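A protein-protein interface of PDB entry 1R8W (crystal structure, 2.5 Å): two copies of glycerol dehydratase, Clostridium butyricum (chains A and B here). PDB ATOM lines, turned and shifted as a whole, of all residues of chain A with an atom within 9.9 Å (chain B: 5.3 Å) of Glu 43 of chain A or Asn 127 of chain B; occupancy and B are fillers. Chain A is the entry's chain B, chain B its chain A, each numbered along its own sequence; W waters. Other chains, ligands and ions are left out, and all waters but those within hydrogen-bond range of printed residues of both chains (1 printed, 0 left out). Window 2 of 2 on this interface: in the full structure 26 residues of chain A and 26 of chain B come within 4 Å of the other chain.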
ATOM      1  N   ILE A  35       2.139 -15.704 -12.799  1.00  0.00           N
ATOM      2  CA  ILE A  35       3.485 -15.144 -12.743  1.00  0.00           C
ATOM      3  C   ILE A  35       4.219 -15.548 -11.459  1.00  0.00           C
ATOM      4  O   ILE A  35       5.432 -15.771 -11.478  1.00  0.00           O
ATOM      5  CB  ILE A  35       3.467 -13.591 -12.913  1.00  0.00           C
ATOM      6  CG1 ILE A  35       4.880 -13.099 -13.219  1.00  0.00           C
ATOM      7  CG2 ILE A  35       2.923 -12.913 -11.664  1.00  0.00           C
ATOM      8  CD1 ILE A  35       4.942 -11.661 -13.656  1.00  0.00           C
ATOM      9  N   THR A  36       3.477 -15.660 -10.358  1.00  0.00           N
ATOM     10  CA  THR A  36       4.028 -16.072  -9.059  1.00  0.00           C
ATOM     11  C   THR A  36       4.483 -17.535  -9.162  1.00  0.00           C
ATOM     12  O   THR A  36       5.548 -17.931  -8.674  1.00  0.00           O
ATOM     13  CB  THR A  36       2.946 -15.969  -7.964  1.00  0.00           C
ATOM     14  OG1 THR A  36       2.549 -14.602  -7.816  1.00  0.00           O
ATOM     15  CG2 THR A  36       3.458 -16.490  -6.640  1.00  0.00           C
ATOM     16  N   GLU A  37       3.642 -18.328  -9.808  1.00  0.00           N
ATOM     17  CA  GLU A  37       3.882 -19.742 -10.033  1.00  0.00           C
ATOM     18  C   GLU A  37       5.217 -19.913 -10.766  1.00  0.00           C
ATOM     19  O   GLU A  37       6.106 -20.628 -10.302  1.00  0.00           O
ATOM     20  CB  GLU A  37       2.733 -20.282 -10.879  1.00  0.00           C
ATOM     21  CG  GLU A  37       2.463 -21.754 -10.789  1.00  0.00           C
ATOM     22  CD  GLU A  37       1.170 -22.107 -11.495  1.00  0.00           C
ATOM     23  OE1 GLU A  37       0.123 -21.539 -11.114  1.00  0.00           O
ATOM     24  OE2 GLU A  37       1.198 -22.938 -12.430  1.00  0.00           O
ATOM     25  N   SER A  38       5.349 -19.243 -11.909  1.00  0.00           N
ATOM     26  CA  SER A  38       6.563 -19.306 -12.717  1.00  0.00           C
ATOM     27  C   SER A  38       7.810 -18.826 -11.978  1.00  0.00           C
ATOM     28  O   SER A  38       8.851 -19.486 -12.014  1.00  0.00           O
ATOM     29  CB  SER A  38       6.390 -18.478 -13.986  1.00  0.00           C
ATOM     30  OG  SER A  38       7.622 -18.350 -14.661  1.00  0.00           O
ATOM     31  N   PHE A  39       7.714 -17.675 -11.317  1.00  0.00           N
ATOM     32  CA  PHE A  39       8.852 -17.138 -10.574  1.00  0.00           C
ATOM     33  C   PHE A  39       9.356 -18.086  -9.488  1.00  0.00           C
ATOM     34  O   PHE A  39      10.551 -18.126  -9.200  1.00  0.00           O
ATOM     35  CB  PHE A  39       8.502 -15.773  -9.962  1.00  0.00           C
ATOM     36  CG  PHE A  39       8.964 -14.603 -10.792  1.00  0.00           C
ATOM     37  CD1 PHE A  39       8.506 -14.432 -12.098  1.00  0.00           C
ATOM     38  CD2 PHE A  39       9.895 -13.701 -10.284  1.00  0.00           C
ATOM     39  CE1 PHE A  39       8.973 -13.381 -12.887  1.00  0.00           C
ATOM     40  CE2 PHE A  39      10.365 -12.653 -11.062  1.00  0.00           C
ATOM     41  CZ  PHE A  39       9.903 -12.492 -12.368  1.00  0.00           C
ATOM     42  N   LYS A  40       8.455 -18.849  -8.882  1.00  0.00           N
ATOM     43  CA  LYS A  40       8.872 -19.788  -7.851  1.00  0.00           C
ATOM     44  C   LYS A  40       9.788 -20.858  -8.431  1.00  0.00           C
ATOM     45  O   LYS A  40      10.637 -21.401  -7.732  1.00  0.00           O
ATOM     46  CB  LYS A  40       7.654 -20.450  -7.196  1.00  0.00           C
ATOM     47  CG  LYS A  40       6.960 -19.564  -6.168  1.00  0.00           C
ATOM     48  CD  LYS A  40       5.746 -20.236  -5.548  1.00  0.00           C
ATOM     49  CE  LYS A  40       5.095 -19.319  -4.516  1.00  0.00           C
ATOM     50  NZ  LYS A  40       3.809 -19.858  -3.989  1.00  0.00           N
ATOM     51  N   GLN A  41       9.630 -21.139  -9.719  1.00  0.00           N
ATOM     52  CA  GLN A  41      10.434 -22.161 -10.375  1.00  0.00           C
ATOM     53  C   GLN A  41      11.684 -21.665 -11.091  1.00  0.00           C
ATOM     54  O   GLN A  41      12.523 -22.466 -11.486  1.00  0.00           O
ATOM     55  CB  GLN A  41       9.580 -22.913 -11.383  1.00  0.00           C
ATOM     56  CG  GLN A  41       8.304 -23.460 -10.820  1.00  0.00           C
ATOM     57  CD  GLN A  41       7.476 -24.135 -11.885  1.00  0.00           C
ATOM     58  OE1 GLN A  41       7.328 -23.610 -12.992  1.00  0.00           O
ATOM     59  NE2 GLN A  41       6.921 -25.301 -11.561  1.00  0.00           N
ATOM     60  N   THR A  42      11.812 -20.356 -11.269  1.00  0.00           N
ATOM     61  CA  THR A  42      12.963 -19.808 -11.974  1.00  0.00           C
ATOM     62  C   THR A  42      13.908 -19.036 -11.067  1.00  0.00           C
ATOM     63  O   THR A  42      14.753 -18.286 -11.538  1.00  0.00           O
ATOM     64  CB  THR A  42      12.503 -18.881 -13.098  1.00  0.00           C
ATOM     65  OG1 THR A  42      11.679 -17.850 -12.546  1.00  0.00           O
ATOM     66  CG2 THR A  42      11.701 -19.656 -14.127  1.00  0.00           C
ATOM     67  N   GLU A  43      13.769 -19.241  -9.764  1.00  0.00           N
ATOM     68  CA  GLU A  43      14.586 -18.557  -8.771  1.00  0.00           C
ATOM     69  C   GLU A  43      16.071 -18.439  -9.125  1.00  0.00           C
ATOM     70  O   GLU A  43      16.700 -17.414  -8.851  1.00  0.00           O
ATOM     71  CB  GLU A  43      14.443 -19.270  -7.428  1.00  0.00           C
ATOM     72  CG  GLU A  43      14.534 -18.367  -6.212  1.00  0.00           C
ATOM     73  CD  GLU A  43      13.338 -17.446  -6.077  1.00  0.00           C
ATOM     74  OE1 GLU A  43      12.195 -17.946  -6.040  1.00  0.00           O
ATOM     75  OE2 GLU A  43      13.545 -16.220  -6.001  1.00  0.00           O
ATOM     76  N   GLY A  44      16.633 -19.477  -9.743  1.00  0.00           N
ATOM     77  CA  GLY A  44      18.048 -19.458 -10.085  1.00  0.00           C
ATOM     78  C   GLY A  44      18.413 -19.019 -11.490  1.00  0.00           C
ATOM     79  O   GLY A  44      19.518 -19.285 -11.960  1.00  0.00           O
ATOM     80  N   GLN A  45      17.496 -18.328 -12.153  1.00  0.00           N
ATOM     81  CA  GLN A  45      17.707 -17.853 -13.514  1.00  0.00           C
ATOM     82  C   GLN A  45      17.923 -16.333 -13.539  1.00  0.00           C
ATOM     83  O   GLN A  45      17.507 -15.621 -12.622  1.00  0.00           O
ATOM     84  CB  GLN A  45      16.475 -18.195 -14.355  1.00  0.00           C
ATOM     85  CG  GLN A  45      16.771 -18.550 -15.787  1.00  0.00           C
ATOM     86  CD  GLN A  45      17.150 -20.005 -15.954  1.00  0.00           C
ATOM     87  OE1 GLN A  45      17.790 -20.380 -16.936  1.00  0.00           O
ATOM     88  NE2 GLN A  45      16.747 -20.836 -15.000  1.00  0.00           N
ATOM     89  N   PRO A  46      18.588 -15.816 -14.584  1.00  0.00           N
ATOM     90  CA  PRO A  46      18.813 -14.368 -14.668  1.00  0.00           C
ATOM     91  C   PRO A  46      17.454 -13.690 -14.840  1.00  0.00           C
ATOM     92  O   PRO A  46      16.533 -14.282 -15.403  1.00  0.00           O
ATOM     93  CB  PRO A  46      19.671 -14.220 -15.921  1.00  0.00           C
ATOM     94  CG  PRO A  46      20.373 -15.524 -16.017  1.00  0.00           C
ATOM     95  CD  PRO A  46      19.308 -16.520 -15.656  1.00  0.00           C
ATOM     96  N   ALA A  47      17.335 -12.452 -14.374  1.00  0.00           N
ATOM     97  CA  ALA A  47      16.086 -11.703 -14.466  1.00  0.00           C
ATOM     98  C   ALA A  47      15.436 -11.713 -15.853  1.00  0.00           C
ATOM     99  O   ALA A  47      14.224 -11.889 -15.977  1.00  0.00           O
ATOM    100  CB  ALA A  47      16.313 -10.263 -14.013  1.00  0.00           C
ATOM    101  N   LEU A  49      15.654 -13.930 -18.222  1.00  0.00           N
ATOM    102  CA  LEU A  49      15.106 -15.248 -18.538  1.00  0.00           C
ATOM    103  C   LEU A  49      13.850 -15.489 -17.696  1.00  0.00           C
ATOM    104  O   LEU A  49      12.895 -16.115 -18.153  1.00  0.00           O
ATOM    105  CB  LEU A  49      16.128 -16.354 -18.245  1.00  0.00           C
ATOM    106  CG  LEU A  49      16.755 -17.172 -19.389  1.00  0.00           C
ATOM    107  CD1 LEU A  49      15.780 -17.293 -20.552  1.00  0.00           C
ATOM    108  CD2 LEU A  49      18.035 -16.511 -19.854  1.00  0.00           C
ATOM    109  N   ARG A  50      13.865 -15.001 -16.461  1.00  0.00           N
ATOM    110  CA  ARG A  50      12.722 -15.142 -15.566  1.00  0.00           C
ATOM    111  C   ARG A  50      11.519 -14.427 -16.185  1.00  0.00           C
ATOM    112  O   ARG A  50      10.394 -14.935 -16.159  1.00  0.00           O
ATOM    113  CB  ARG A  50      13.040 -14.521 -14.203  1.00  0.00           C
ATOM    114  CG  ARG A  50      14.105 -15.256 -13.417  1.00  0.00           C
ATOM    115  CD  ARG A  50      13.528 -15.790 -12.126  1.00  0.00           C
ATOM    116  NE  ARG A  50      13.651 -14.854 -11.017  1.00  0.00           N
ATOM    117  CZ  ARG A  50      13.093 -15.040  -9.825  1.00  0.00           C
ATOM    118  NH1 ARG A  50      12.365 -16.125  -9.596  1.00  0.00           N
ATOM    119  NH2 ARG A  50      13.276 -14.153  -8.856  1.00  0.00           N
ATOM    120  N   ARG A  51      11.769 -13.242 -16.736  1.00  0.00           N
ATOM    121  CA  ARG A  51      10.719 -12.460 -17.368  1.00  0.00           C
ATOM    122  C   ARG A  51      10.181 -13.170 -18.609  1.00  0.00           C
ATOM    123  O   ARG A  51       8.973 -13.177 -18.847  1.00  0.00           O
ATOM    124  CB  ARG A  51      11.245 -11.075 -17.752  1.00  0.00           C
ATOM    125  CG  ARG A  51      11.518 -10.156 -16.569  1.00  0.00           C
ATOM    126  CD  ARG A  51      10.263  -9.887 -15.747  1.00  0.00           C
ATOM    127  NE  ARG A  51       9.117  -9.566 -16.595  1.00  0.00           N
ATOM    128  CZ  ARG A  51       7.942  -9.135 -16.144  1.00  0.00           C
ATOM    129  NH1 ARG A  51       7.746  -8.962 -14.841  1.00  0.00           N
ATOM    130  NH2 ARG A  51       6.960  -8.888 -16.996  1.00  0.00           N
ATOM    131  N   LEU A  53      10.384 -16.518 -19.333  1.00  0.00           N
ATOM    132  CA  LEU A  53       9.710 -17.738 -18.904  1.00  0.00           C
ATOM    133  C   LEU A  53       8.366 -17.437 -18.242  1.00  0.00           C
ATOM    134  O   LEU A  53       7.428 -18.232 -18.338  1.00  0.00           O
ATOM    135  CB  LEU A  53      10.609 -18.525 -17.941  1.00  0.00           C
ATOM    136  CG  LEU A  53      11.483 -19.671 -18.475  1.00  0.00           C
ATOM    137  CD1 LEU A  53      11.515 -19.680 -19.990  1.00  0.00           C
ATOM    138  CD2 LEU A  53      12.879 -19.539 -17.901  1.00  0.00           C
ATOM    139  N   TYR A 125       4.503 -14.267  -1.366  1.00  0.00           N
ATOM    140  CA  TYR A 125       5.697 -14.544  -2.153  1.00  0.00           C
ATOM    141  C   TYR A 125       6.483 -13.315  -2.600  1.00  0.00           C
ATOM    142  O   TYR A 125       7.709 -13.289  -2.480  1.00  0.00           O
ATOM    143  CB  TYR A 125       5.350 -15.360  -3.400  1.00  0.00           C
ATOM    144  CG  TYR A 125       6.543 -15.546  -4.309  1.00  0.00           C
ATOM    145  CD1 TYR A 125       7.595 -16.382  -3.940  1.00  0.00           C
ATOM    146  CD2 TYR A 125       6.663 -14.822  -5.499  1.00  0.00           C
ATOM    147  CE1 TYR A 125       8.738 -16.488  -4.724  1.00  0.00           C
ATOM    148  CE2 TYR A 125       7.810 -14.921  -6.293  1.00  0.00           C
ATOM    149  CZ  TYR A 125       8.842 -15.755  -5.895  1.00  0.00           C
ATOM    150  OH  TYR A 125       9.989 -15.845  -6.644  1.00  0.00           O
ATOM    151  N   TRP A 126       5.786 -12.307  -3.123  1.00  0.00           N
ATOM    152  CA  TRP A 126       6.451 -11.103  -3.622  1.00  0.00           C
ATOM    153  C   TRP A 126       6.995 -10.111  -2.603  1.00  0.00           C
ATOM    154  O   TRP A 126       7.518  -9.065  -2.985  1.00  0.00           O
ATOM    155  CB  TRP A 126       5.541 -10.354  -4.602  1.00  0.00           C
ATOM    156  CG  TRP A 126       5.302 -11.111  -5.875  1.00  0.00           C
ATOM    157  CD1 TRP A 126       4.270 -11.968  -6.141  1.00  0.00           C
ATOM    158  CD2 TRP A 126       6.145 -11.128  -7.036  1.00  0.00           C
ATOM    159  NE1 TRP A 126       4.419 -12.517  -7.391  1.00  0.00           N
ATOM    160  CE2 TRP A 126       5.561 -12.022  -7.963  1.00  0.00           C
ATOM    161  CE3 TRP A 126       7.339 -10.479  -7.382  1.00  0.00           C
ATOM    162  CZ2 TRP A 126       6.130 -12.283  -9.217  1.00  0.00           C
ATOM    163  CZ3 TRP A 126       7.906 -10.739  -8.631  1.00  0.00           C
ATOM    164  CH2 TRP A 126       7.298 -11.635  -9.531  1.00  0.00           C
ATOM    165  N   ASN A 127       6.900 -10.428  -1.315  1.00  0.00           N
ATOM    166  CA  ASN A 127       7.407  -9.511  -0.302  1.00  0.00           C
ATOM    167  C   ASN A 127       8.906  -9.247  -0.469  1.00  0.00           C
ATOM    168  O   ASN A 127       9.728 -10.145  -0.290  1.00  0.00           O
ATOM    169  CB  ASN A 127       7.135 -10.042   1.111  1.00  0.00           C
ATOM    170  CG  ASN A 127       7.632  -9.088   2.192  1.00  0.00           C
ATOM    171  OD1 ASN A 127       7.211  -7.936   2.257  1.00  0.00           O
ATOM    172  ND2 ASN A 127       8.539  -9.562   3.033  1.00  0.00           N
ATOM    173  N   GLY A 128       9.245  -8.005  -0.810  1.00  0.00           N
ATOM    174  CA  GLY A 128      10.633  -7.621  -0.999  1.00  0.00           C
ATOM    175  C   GLY A 128      11.214  -7.985  -2.357  1.00  0.00           C
ATOM    176  O   GLY A 128      12.383  -7.715  -2.625  1.00  0.00           O
ATOM    177  N   LYS A 129      10.404  -8.579  -3.225  1.00  0.00           N
ATOM    178  CA  LYS A 129      10.886  -8.996  -4.535  1.00  0.00           C
ATOM    179  C   LYS A 129      10.375  -8.152  -5.693  1.00  0.00           C
ATOM    180  O   LYS A 129      10.591  -8.489  -6.855  1.00  0.00           O
ATOM    181  CB  LYS A 129      10.512 -10.459  -4.765  1.00  0.00           C
ATOM    182  CG  LYS A 129      10.890 -11.348  -3.600  1.00  0.00           C
ATOM    183  CD  LYS A 129      10.621 -12.801  -3.905  1.00  0.00           C
ATOM    184  CE  LYS A 129      10.930 -13.662  -2.699  1.00  0.00           C
ATOM    185  NZ  LYS A 129      10.945 -15.093  -3.088  1.00  0.00           N
ATOM    186  N   ARG A 516      15.179  -5.727 -12.054  1.00  0.00           N
ATOM    187  CA  ARG A 516      14.209  -6.776 -11.773  1.00  0.00           C
ATOM    188  C   ARG A 516      13.137  -7.017 -12.823  1.00  0.00           C
ATOM    189  O   ARG A 516      12.464  -8.041 -12.784  1.00  0.00           O
ATOM    190  CB  ARG A 516      13.546  -6.522 -10.419  1.00  0.00           C
ATOM    191  CG  ARG A 516      14.513  -6.643  -9.267  1.00  0.00           C
ATOM    192  CD  ARG A 516      13.841  -6.544  -7.910  1.00  0.00           C
ATOM    193  NE  ARG A 516      14.803  -6.867  -6.861  1.00  0.00           N
ATOM    194  CZ  ARG A 516      14.503  -6.989  -5.574  1.00  0.00           C
ATOM    195  NH1 ARG A 516      13.257  -6.811  -5.166  1.00  0.00           N
ATOM    196  NH2 ARG A 516      15.450  -7.298  -4.700  1.00  0.00           N
ATOM    197  N   LYS B  92      23.453 -27.896  -1.811  1.00  0.00           N
ATOM    198  CA  LYS B  92      22.767 -29.154  -2.063  1.00  0.00           C
ATOM    199  C   LYS B  92      23.713 -30.342  -1.857  1.00  0.00           C
ATOM    200  O   LYS B  92      23.290 -31.402  -1.404  1.00  0.00           O
ATOM    201  CB  LYS B  92      22.187 -29.181  -3.478  1.00  0.00           C
ATOM    202  CG  LYS B  92      21.029 -28.212  -3.682  1.00  0.00           C
ATOM    203  CD  LYS B  92      20.510 -28.263  -5.114  1.00  0.00           C
ATOM    204  CE  LYS B  92      19.554 -27.111  -5.418  1.00  0.00           C
ATOM    205  NZ  LYS B  92      18.365 -27.129  -4.525  1.00  0.00           N
ATOM    206  N   VAL B 122      17.991 -23.871   6.161  1.00  0.00           N
ATOM    207  CA  VAL B 122      19.008 -23.288   5.304  1.00  0.00           C
ATOM    208  C   VAL B 122      18.872 -23.806   3.875  1.00  0.00           C
ATOM    209  O   VAL B 122      18.793 -23.019   2.932  1.00  0.00           O
ATOM    210  CB  VAL B 122      20.416 -23.619   5.833  1.00  0.00           C
ATOM    211  CG1 VAL B 122      21.467 -23.003   4.932  1.00  0.00           C
ATOM    212  CG2 VAL B 122      20.564 -23.113   7.264  1.00  0.00           C
ATOM    213  N   PHE B 123      18.838 -25.128   3.726  1.00  0.00           N
ATOM    214  CA  PHE B 123      18.720 -25.766   2.418  1.00  0.00           C
ATOM    215  C   PHE B 123      17.469 -25.313   1.697  1.00  0.00           C
ATOM    216  O   PHE B 123      17.494 -25.005   0.507  1.00  0.00           O
ATOM    217  CB  PHE B 123      18.658 -27.291   2.558  1.00  0.00           C
ATOM    218  CG  PHE B 123      19.891 -27.901   3.150  1.00  0.00           C
ATOM    219  CD1 PHE B 123      19.791 -28.866   4.148  1.00  0.00           C
ATOM    220  CD2 PHE B 123      21.157 -27.528   2.703  1.00  0.00           C
ATOM    221  CE1 PHE B 123      20.932 -29.450   4.694  1.00  0.00           C
ATOM    222  CE2 PHE B 123      22.305 -28.106   3.242  1.00  0.00           C
ATOM    223  CZ  PHE B 123      22.193 -29.069   4.239  1.00  0.00           C
ATOM    224  N   GLU B 124      16.368 -25.280   2.430  1.00  0.00           N
ATOM    225  CA  GLU B 124      15.091 -24.896   1.861  1.00  0.00           C
ATOM    226  C   GLU B 124      15.047 -23.453   1.379  1.00  0.00           C
ATOM    227  O   GLU B 124      14.473 -23.168   0.331  1.00  0.00           O
ATOM    228  CB  GLU B 124      13.992 -25.138   2.884  1.00  0.00           C
ATOM    229  CG  GLU B 124      12.596 -25.013   2.338  1.00  0.00           C
ATOM    230  CD  GLU B 124      11.566 -25.363   3.385  1.00  0.00           C
ATOM    231  OE1 GLU B 124      11.556 -26.537   3.828  1.00  0.00           O
ATOM    232  OE2 GLU B 124      10.782 -24.465   3.771  1.00  0.00           O
ATOM    233  N   TYR B 125      15.648 -22.542   2.137  1.00  0.00           N
ATOM    234  CA  TYR B 125      15.655 -21.135   1.754  1.00  0.00           C
ATOM    235  C   TYR B 125      16.553 -20.824   0.554  1.00  0.00           C
ATOM    236  O   TYR B 125      16.138 -20.125  -0.374  1.00  0.00           O
ATOM    237  CB  TYR B 125      16.093 -20.248   2.928  1.00  0.00           C
ATOM    238  CG  TYR B 125      16.223 -18.787   2.536  1.00  0.00           C
ATOM    239  CD1 TYR B 125      15.097 -18.038   2.186  1.00  0.00           C
ATOM    240  CD2 TYR B 125      17.477 -18.181   2.421  1.00  0.00           C
ATOM    241  CE1 TYR B 125      15.212 -16.734   1.723  1.00  0.00           C
ATOM    242  CE2 TYR B 125      17.603 -16.870   1.955  1.00  0.00           C
ATOM    243  CZ  TYR B 125      16.465 -16.158   1.604  1.00  0.00           C
ATOM    244  OH  TYR B 125      16.574 -14.888   1.095  1.00  0.00           O
ATOM    245  N   TRP B 126      17.782 -21.338   0.578  1.00  0.00           N
ATOM    246  CA  TRP B 126      18.738 -21.068  -0.491  1.00  0.00           C
ATOM    247  C   TRP B 126      18.504 -21.734  -1.838  1.00  0.00           C
ATOM    248  O   TRP B 126      19.287 -21.546  -2.766  1.00  0.00           O
ATOM    249  CB  TRP B 126      20.153 -21.380  -0.010  1.00  0.00           C
ATOM    250  CG  TRP B 126      20.601 -20.439   1.047  1.00  0.00           C
ATOM    251  CD1 TRP B 126      20.532 -20.624   2.403  1.00  0.00           C
ATOM    252  CD2 TRP B 126      21.129 -19.126   0.847  1.00  0.00           C
ATOM    253  NE1 TRP B 126      20.986 -19.504   3.057  1.00  0.00           N
ATOM    254  CE2 TRP B 126      21.358 -18.568   2.126  1.00  0.00           C
ATOM    255  CE3 TRP B 126      21.431 -18.362  -0.289  1.00  0.00           C
ATOM    256  CZ2 TRP B 126      21.877 -17.274   2.300  1.00  0.00           C
ATOM    257  CZ3 TRP B 126      21.946 -17.078  -0.118  1.00  0.00           C
ATOM    258  CH2 TRP B 126      22.162 -16.549   1.170  1.00  0.00           C
ATOM    259  N   ASN B 127      17.426 -22.497  -1.964  1.00  0.00           N
ATOM    260  CA  ASN B 127      17.151 -23.160  -3.228  1.00  0.00           C
ATOM    261  C   ASN B 127      17.012 -22.150  -4.370  1.00  0.00           C
ATOM    262  O   ASN B 127      16.126 -21.302  -4.351  1.00  0.00           O
ATOM    263  CB  ASN B 127      15.878 -24.003  -3.132  1.00  0.00           C
ATOM    264  CG  ASN B 127      15.596 -24.760  -4.417  1.00  0.00           C
ATOM    265  OD1 ASN B 127      16.360 -25.637  -4.810  1.00  0.00           O
ATOM    266  ND2 ASN B 127      14.508 -24.407  -5.088  1.00  0.00           N
ATOM    267  N   GLY B 128      17.899 -22.249  -5.354  1.00  0.00           N
ATOM    268  CA  GLY B 128      17.865 -21.354  -6.498  1.00  0.00           C
ATOM    269  C   GLY B 128      18.448 -19.972  -6.251  1.00  0.00           C
ATOM    270  O   GLY B 128      18.512 -19.151  -7.166  1.00  0.00           O
ATOM    271  N   LYS B 129      18.902 -19.714  -5.027  1.00  0.00           N
ATOM    272  CA  LYS B 129      19.437 -18.401  -4.689  1.00  0.00           C
ATOM    273  C   LYS B 129      20.947 -18.333  -4.524  1.00  0.00           C
ATOM    274  O   LYS B 129      21.484 -17.301  -4.113  1.00  0.00           O
ATOM    275  CB  LYS B 129      18.757 -17.900  -3.417  1.00  0.00           C
ATOM    276  CG  LYS B 129      17.245 -17.968  -3.501  1.00  0.00           C
ATOM    277  CD  LYS B 129      16.588 -17.468  -2.232  1.00  0.00           C
ATOM    278  CE  LYS B 129      15.088 -17.684  -2.288  1.00  0.00           C
ATOM    279  NZ  LYS B 129      14.423 -16.978  -1.169  1.00  0.00           N
ATOM    280  N   GLU B 133      24.050 -21.838  -8.756  1.00  0.00           N
ATOM    281  CA  GLU B 133      22.869 -22.044  -9.582  1.00  0.00           C
ATOM    282  C   GLU B 133      22.734 -20.983 -10.683  1.00  0.00           C
ATOM    283  O   GLU B 133      22.278 -21.288 -11.787  1.00  0.00           O
ATOM    284  CB  GLU B 133      21.616 -22.096  -8.695  1.00  0.00           C
ATOM    285  CG  GLU B 133      21.603 -23.330  -7.797  1.00  0.00           C
ATOM    286  CD  GLU B 133      20.675 -23.210  -6.602  1.00  0.00           C
ATOM    287  OE1 GLU B 133      19.637 -23.903  -6.579  1.00  0.00           O
ATOM    288  OE2 GLU B 133      20.989 -22.425  -5.681  1.00  0.00           O
ATOM    289  N   ARG B 516      25.542 -12.001  -7.404  1.00  0.00           N
ATOM    290  CA  ARG B 516      24.960 -12.417  -6.133  1.00  0.00           C
ATOM    291  C   ARG B 516      25.874 -12.406  -4.916  1.00  0.00           C
ATOM    292  O   ARG B 516      25.391 -12.530  -3.791  1.00  0.00           O
ATOM    293  CB  ARG B 516      24.346 -13.809  -6.276  1.00  0.00           C
ATOM    294  CG  ARG B 516      23.143 -13.837  -7.188  1.00  0.00           C
ATOM    295  CD  ARG B 516      22.506 -15.209  -7.264  1.00  0.00           C
ATOM    296  NE  ARG B 516      21.265 -15.133  -8.025  1.00  0.00           N
ATOM    297  CZ  ARG B 516      20.407 -16.135  -8.175  1.00  0.00           C
ATOM    298  NH1 ARG B 516      20.650 -17.314  -7.614  1.00  0.00           N
ATOM    299  NH2 ARG B 516      19.292 -15.948  -8.872  1.00  0.00           N
HETATM  300  O   HOH W   1      17.972 -13.628 -10.677  1.00  0.00           O
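Of chain B, only Asn 127 (3.8 Å), Gly 128 (3.0 Å), Lys 129 (3.9 Å) and Arg 516 (3.0 Å) come within 4 Å of Glu 43 of chain A.
Of chain A, only Glu 43 (3.8 Å) comes within 4 Å of Asn 127 of chain B.
Gly 128 of chain B touches two residues of chain A.
Of the printed residues of chain A, Glu 133 of chain B touches Gly 44.
Printed residues of chain A within 4 Å of Lys 129 of chain B: Glu 43.
Of the printed residues of chain A, Arg 516 of chain B touches Glu 43 (3.0 Å) and Gly 44 (3.9 Å).
Trp 126 of chain B touches none of the printed residues of chain A.
Arg 51 of chain A touches none of the printed residues of chain B.
The nearest printed residue of chain B that does not touch Glu 43 of chain A is Tyr 125 of chain B (6.3 Å).
The nearest residue of chain A that does not touch Asn 127 of chain B is Lys 40 of chain A (5.6 Å).
The nearest printed residue of chain A that does not touch Lys 129 of chain B is Lys 129 of chain A (4.4 Å).
Positions printed for both chains: 125, 126, 127, 128, 129 and 516.
Of the 7 pairs that touch across the chains among the printed residues, none has its exchanged pair printed and touching as well.
Water W1 bridges O of Gln 45 of chain A (2.8 Å) and NH2 of Arg 516 of chain B (3.2 Å).
Among the printed residues, merely in contact across the chains: Glu 43 of chain A with Asn 127 of chain B (3.8 Å), Glu 43 of chain A with Lys 129 of chain B (3.9 Å) and Gly 44 of chain A with Arg 516 of chain B (3.9 Å).
Of the 23 printed residues of chain A, 2 touch a printed residue of chain B.
Among the printed residues, 7 pairs touch across the chains.
Among the printed residues, no Asp or Glu carboxylate lies within 4 Å of a Lys or Arg side-chain nitrogen of the other chain.
OD1 of Asn 127 of chain B is in hydrogen-bond range of NZ of Lys 92 of chain B, at 2.5 Å.
The backbone NH (N) of Gly 128 of chain B is in hydrogen-bond range of the side-chain carboxylate (OE1) of Glu 133 of chain B, 2.7 Å away.
The backbone carbonyl oxygen of Gly 128 of chain B is in hydrogen-bond range of the guanidinium group of Arg 516 of chain B (2.9 Å).
The side-chain carboxylate of Glu 133 of chain B lies within hydrogen-bond range of the backbone NH of Lys 129 of chain B (3.5 Å).
OE2 of Glu 43 of chain A lies within salt-bridge range of NH2 of Arg 50 of chain A (3.5 Å).
The side-chain hydroxyl (OH) of Tyr 125 of chain A lies within hydrogen-bond range of the side-chain carboxylate (OE1) of Glu 43 of chain A (3.1 Å).
O of Gly 128 of chain B lies close to N of Gly 44 of chain A (3.2 Å).
NH2 of Arg 516 of chain B lies within hydrogen-bond range of O of Glu 43 of chain A.
The backbone carbonyl oxygen (O) of Gly 128 of chain B lies close to the backbone carbonyl oxygen (O) of Glu 43 of chain A (3.0 Å).
O of Gly 44 of chain A sits close to O of Glu 133 of chain B (3.4 Å).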
